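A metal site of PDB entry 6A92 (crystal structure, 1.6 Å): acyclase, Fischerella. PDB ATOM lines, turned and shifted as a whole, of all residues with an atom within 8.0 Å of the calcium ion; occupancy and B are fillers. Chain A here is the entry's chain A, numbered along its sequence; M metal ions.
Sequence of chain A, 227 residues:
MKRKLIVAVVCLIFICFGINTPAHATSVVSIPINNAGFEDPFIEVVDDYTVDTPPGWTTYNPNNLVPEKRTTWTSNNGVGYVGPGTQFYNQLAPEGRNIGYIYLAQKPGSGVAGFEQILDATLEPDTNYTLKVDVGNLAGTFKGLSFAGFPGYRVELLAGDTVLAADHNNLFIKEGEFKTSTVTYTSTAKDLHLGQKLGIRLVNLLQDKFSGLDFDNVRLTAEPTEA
OD1 of Asn 35 is in hydrogen-bond range of N of Glu 39, 3.1 Å away. The side-chain amide nitrogen (ND2) of Asn 98 sits at hydrogen-bond distance from the backbone carbonyl oxygen (O) of Phe 38, at 3.0 Å. The backbone NH (N) of Arg 97 lies within hydrogen-bond range of the side-chain carboxylate (OE1) of Glu 39 (2.9 Å).
Five residues have an atom within 4 Å of the calcium ion: Gly 37, Glu 39, Glu 95, Asn 98 and Asp 216. The nearest printed residue that does not touch the calcium ion is Gly 96 (4.3 Å).
The calcium ion is bound by the backbone carbonyl oxygen (O) of Asn 98 (2.3 Å), the backbone carbonyl oxygen (O) of Glu 95 (2.4 Å), the side-chain carboxylate (OD1) of Asp 216 (2.4 Å), the backbone carbonyl oxygen (O) of Gly 37 (2.4 Å), the side-chain carboxylate (OE2) of Glu 39 (2.4 Å), the side-chain carboxylate (OE1) of Glu 95 (2.4 Å) and the side-chain carboxylate (OD2) of Asp 216 (2.7 Å).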
ATOM      1  N   ASN A  35      -1.354  33.606  -3.977  1.00  0.00           N
ATOM      2  CA  ASN A  35      -1.052  32.274  -4.563  1.00  0.00           C
ATOM      3  C   ASN A  35      -1.310  31.169  -3.536  1.00  0.00           C
ATOM      4  O   ASN A  35      -0.538  30.241  -3.367  1.00  0.00           O
ATOM      5  CB  ASN A  35       0.373  32.218  -5.133  1.00  0.00           C
ATOM      6  CG  ASN A  35       0.573  31.159  -6.190  1.00  0.00           C
ATOM      7  OD1 ASN A  35      -0.383  30.652  -6.775  1.00  0.00           O
ATOM      8  ND2 ASN A  35       1.836  30.807  -6.396  1.00  0.00           N
ATOM      9  N   ALA A  36      -2.481  31.270  -2.883  1.00  0.00           N
ATOM     10  CA  ALA A  36      -2.795  30.402  -1.736  1.00  0.00           C
ATOM     11  C   ALA A  36      -2.991  28.943  -2.126  1.00  0.00           C
ATOM     12  O   ALA A  36      -2.910  28.093  -1.251  1.00  0.00           O
ATOM     13  CB  ALA A  36      -4.007  30.960  -1.018  1.00  0.00           C
ATOM     14  N   GLY A  37      -3.289  28.669  -3.417  1.00  0.00           N
ATOM     15  CA  GLY A  37      -3.416  27.314  -3.842  1.00  0.00           C
ATOM     16  C   GLY A  37      -2.339  26.925  -4.848  1.00  0.00           C
ATOM     17  O   GLY A  37      -2.454  25.875  -5.515  1.00  0.00           O
ATOM     18  N   PHE A  38      -1.254  27.699  -4.876  1.00  0.00           N
ATOM     19  CA  PHE A  38      -0.081  27.387  -5.753  1.00  0.00           C
ATOM     20  C   PHE A  38      -0.531  27.265  -7.209  1.00  0.00           C
ATOM     21  O   PHE A  38       0.149  26.538  -7.928  1.00  0.00           O
ATOM     22  CB  PHE A  38       0.631  26.121  -5.247  1.00  0.00           C
ATOM     23  CG  PHE A  38       1.110  26.289  -3.821  1.00  0.00           C
ATOM     24  CD1 PHE A  38       2.252  27.022  -3.544  1.00  0.00           C
ATOM     25  CD2 PHE A  38       0.469  25.681  -2.759  1.00  0.00           C
ATOM     26  CE1 PHE A  38       2.695  27.217  -2.252  1.00  0.00           C
ATOM     27  CE2 PHE A  38       0.911  25.870  -1.454  1.00  0.00           C
ATOM     28  CZ  PHE A  38       2.010  26.631  -1.203  1.00  0.00           C
ATOM     29  N   GLU A  39      -1.563  27.958  -7.629  1.00  0.00           N
ATOM     30  CA  GLU A  39      -2.055  27.824  -8.994  1.00  0.00           C
ATOM     31  C   GLU A  39      -1.159  28.572  -9.984  1.00  0.00           C
ATOM     32  O   GLU A  39      -1.271  28.322 -11.196  1.00  0.00           O
ATOM     33  CB  GLU A  39      -3.516  28.235  -9.058  1.00  0.00           C
ATOM     34  CG  GLU A  39      -4.415  27.271  -8.304  1.00  0.00           C
ATOM     35  CD  GLU A  39      -4.320  25.822  -8.764  1.00  0.00           C
ATOM     36  OE1 GLU A  39      -4.557  25.597 -10.007  1.00  0.00           O
ATOM     37  OE2 GLU A  39      -3.987  24.939  -7.969  1.00  0.00           O
ATOM     38  N   ASP A  40      -0.286  29.459  -9.509  1.00  0.00           N
ATOM     39  CA  ASP A  40       0.757  30.064 -10.362  1.00  0.00           C
ATOM     40  C   ASP A  40       2.092  29.426 -10.013  1.00  0.00           C
ATOM     41  O   ASP A  40       2.450  29.326  -8.856  1.00  0.00           O
ATOM     42  CB  ASP A  40       0.892  31.577 -10.193  1.00  0.00           C
ATOM     43  CG  ASP A  40      -0.117  32.423 -10.964  1.00  0.00           C
ATOM     44  OD1 ASP A  40      -0.925  31.826 -11.711  1.00  0.00           O
ATOM     45  OD2 ASP A  40      -0.080  33.663 -10.819  1.00  0.00           O
ATOM     46  N   GLY A  80       3.610  21.681  -8.441  1.00  0.00           N
ATOM     47  CA  GLY A  80       3.426  20.474  -9.231  1.00  0.00           C
ATOM     48  C   GLY A  80       1.974  20.317  -9.623  1.00  0.00           C
ATOM     49  O   GLY A  80       1.075  20.626  -8.817  1.00  0.00           O
ATOM     50  N   ALA A  93      -5.423  17.217  -6.929  1.00  0.00           N
ATOM     51  CA  ALA A  93      -5.044  18.287  -6.033  1.00  0.00           C
ATOM     52  C   ALA A  93      -6.260  18.627  -5.180  1.00  0.00           C
ATOM     53  O   ALA A  93      -7.387  18.638  -5.666  1.00  0.00           O
ATOM     54  CB  ALA A  93      -4.587  19.508  -6.788  1.00  0.00           C
ATOM     55  N   PRO A  94      -6.059  18.997  -3.890  1.00  0.00           N
ATOM     56  CA  PRO A  94      -7.192  19.430  -3.076  1.00  0.00           C
ATOM     57  C   PRO A  94      -7.936  20.630  -3.681  1.00  0.00           C
ATOM     58  O   PRO A  94      -9.125  20.767  -3.440  1.00  0.00           O
ATOM     59  CB  PRO A  94      -6.517  19.837  -1.769  1.00  0.00           C
ATOM     60  CG  PRO A  94      -5.346  18.877  -1.674  1.00  0.00           C
ATOM     61  CD  PRO A  94      -4.833  18.783  -3.106  1.00  0.00           C
ATOM     62  N   GLU A  95      -7.227  21.479  -4.415  1.00  0.00           N
ATOM     63  CA  GLU A  95      -7.805  22.674  -5.005  1.00  0.00           C
ATOM     64  C   GLU A  95      -7.140  22.919  -6.351  1.00  0.00           C
ATOM     65  O   GLU A  95      -5.900  22.865  -6.460  1.00  0.00           O
ATOM     66  CB  GLU A  95      -7.639  23.862  -4.046  1.00  0.00           C
ATOM     67  CG  GLU A  95      -8.076  25.199  -4.572  1.00  0.00           C
ATOM     68  CD  GLU A  95      -7.054  25.982  -5.385  1.00  0.00           C
ATOM     69  OE1 GLU A  95      -5.868  25.626  -5.336  1.00  0.00           O
ATOM     70  OE2 GLU A  95      -7.471  26.980  -6.004  1.00  0.00           O
ATOM     71  N   GLY A  96      -7.943  23.178  -7.374  1.00  0.00           N
ATOM     72  CA  GLY A  96      -7.307  23.579  -8.675  1.00  0.00           C
ATOM     73  C   GLY A  96      -6.504  22.427  -9.276  1.00  0.00           C
ATOM     74  O   GLY A  96      -6.787  21.248  -9.058  1.00  0.00           O
ATOM     75  N   ARG A  97      -5.439  22.825  -9.979  1.00  0.00           N
ATOM     76  CA  ARG A  97      -4.567  21.913 -10.654  1.00  0.00           C
ATOM     77  C   ARG A  97      -3.342  21.545  -9.848  1.00  0.00           C
ATOM     78  O   ARG A  97      -2.889  20.399  -9.923  1.00  0.00           O
ATOM     79  CB  ARG A  97      -4.075  22.613 -11.923  1.00  0.00           C
ATOM     80  CG  ARG A  97      -5.173  22.829 -12.954  1.00  0.00           C
ATOM     81  CD  ARG A  97      -4.726  23.668 -14.134  1.00  0.00           C
ATOM     82  NE  ARG A  97      -3.668  23.053 -14.942  1.00  0.00           N
ATOM     83  CZ  ARG A  97      -3.931  22.346 -16.052  1.00  0.00           C
ATOM     84  NH1 ARG A  97      -5.188  22.137 -16.447  1.00  0.00           N
ATOM     85  NH2 ARG A  97      -2.930  21.902 -16.796  1.00  0.00           N
ATOM     86  N   ASN A  98      -2.823  22.511  -9.066  1.00  0.00           N
ATOM     87  CA  ASN A  98      -1.485  22.431  -8.550  1.00  0.00           C
ATOM     88  C   ASN A  98      -1.431  22.276  -7.031  1.00  0.00           C
ATOM     89  O   ASN A  98      -2.326  22.727  -6.331  1.00  0.00           O
ATOM     90  CB  ASN A  98      -0.689  23.687  -8.852  1.00  0.00           C
ATOM     91  CG  ASN A  98      -0.350  23.916 -10.317  1.00  0.00           C
ATOM     92  OD1 ASN A  98      -0.530  22.999 -11.144  1.00  0.00           O
ATOM     93  ND2 ASN A  98       0.112  25.126 -10.596  1.00  0.00           N
ATOM     94  N   ILE A  99      -0.310  21.731  -6.599  1.00  0.00           N
ATOM     95  CA  ILE A  99       0.152  21.749  -5.214  1.00  0.00           C
ATOM     96  C   ILE A  99       1.494  22.454  -5.149  1.00  0.00           C
ATOM     97  O   ILE A  99       2.127  22.736  -6.128  1.00  0.00           O
ATOM     98  CB  ILE A  99       0.153  20.331  -4.609  1.00  0.00           C
ATOM     99  CG1 ILE A  99       1.137  19.356  -5.289  1.00  0.00           C
ATOM    100  CG2 ILE A  99      -1.272  19.799  -4.677  1.00  0.00           C
ATOM    101  CD1 ILE A  99       2.590  19.637  -5.099  1.00  0.00           C
ATOM    102  N   GLY A 100       1.865  22.819  -3.899  1.00  0.00           N
ATOM    103  CA  GLY A 100       3.224  23.277  -3.592  1.00  0.00           C
ATOM    104  C   GLY A 100       3.990  22.188  -2.885  1.00  0.00           C
ATOM    105  O   GLY A 100       3.466  21.546  -1.995  1.00  0.00           O
ATOM    106  N   PHE A 215       1.723  20.640  -0.134  1.00  0.00           N
ATOM    107  CA  PHE A 215       0.709  21.466   0.511  1.00  0.00           C
ATOM    108  C   PHE A 215      -0.251  22.059  -0.497  1.00  0.00           C
ATOM    109  O   PHE A 215       0.131  22.292  -1.646  1.00  0.00           O
ATOM    110  CB  PHE A 215       1.398  22.612   1.253  1.00  0.00           C
ATOM    111  CG  PHE A 215       2.283  22.186   2.398  1.00  0.00           C
ATOM    112  CD1 PHE A 215       1.725  21.852   3.624  1.00  0.00           C
ATOM    113  CD2 PHE A 215       3.653  22.097   2.269  1.00  0.00           C
ATOM    114  CE1 PHE A 215       2.532  21.489   4.685  1.00  0.00           C
ATOM    115  CE2 PHE A 215       4.454  21.741   3.348  1.00  0.00           C
ATOM    116  CZ  PHE A 215       3.891  21.380   4.537  1.00  0.00           C
ATOM    117  N   ASP A 216      -1.483  22.368  -0.086  1.00  0.00           N
ATOM    118  CA  ASP A 216      -2.395  23.062  -0.969  1.00  0.00           C
ATOM    119  C   ASP A 216      -3.521  23.731  -0.193  1.00  0.00           C
ATOM    120  O   ASP A 216      -3.726  23.435   0.985  1.00  0.00           O
ATOM    121  CB  ASP A 216      -3.011  22.111  -2.002  1.00  0.00           C
ATOM    122  CG  ASP A 216      -3.607  22.756  -3.238  1.00  0.00           C
ATOM    123  OD1 ASP A 216      -3.417  23.976  -3.459  1.00  0.00           O
ATOM    124  OD2 ASP A 216      -4.325  22.042  -3.979  1.00  0.00           O
ATOM    125  N   ASN A 217      -4.161  24.683  -0.851  1.00  0.00           N
ATOM    126  CA  ASN A 217      -5.420  25.276  -0.430  1.00  0.00           C
ATOM    127  C   ASN A 217      -5.255  25.918   0.950  1.00  0.00           C
ATOM    128  O   ASN A 217      -5.987  25.577   1.871  1.00  0.00           O
ATOM    129  CB  ASN A 217      -6.535  24.235  -0.406  1.00  0.00           C
ATOM    130  CG  ASN A 217      -7.902  24.892  -0.326  1.00  0.00           C
ATOM    131  OD1 ASN A 217      -8.070  26.066  -0.676  1.00  0.00           O
ATOM    132  ND2 ASN A 217      -8.907  24.098   0.027  1.00  0.00           N
ATOM    133  N   VAL A 218      -4.309  26.839   1.034  1.00  0.00           N
ATOM    134  CA  VAL A 218      -4.068  27.544   2.306  1.00  0.00           C
ATOM    135  C   VAL A 218      -5.204  28.531   2.504  1.00  0.00           C
ATOM    136  O   VAL A 218      -5.502  29.317   1.622  1.00  0.00           O
ATOM    137  CB  VAL A 218      -2.702  28.272   2.259  1.00  0.00           C
ATOM    138  CG1 VAL A 218      -2.398  28.890   3.618  1.00  0.00           C
ATOM    139  CG2 VAL A 218      -1.578  27.318   1.878  1.00  0.00           C
HETATM  140 CA    CA M   1      -4.047  24.125  -5.736  1.00  0.00          CA
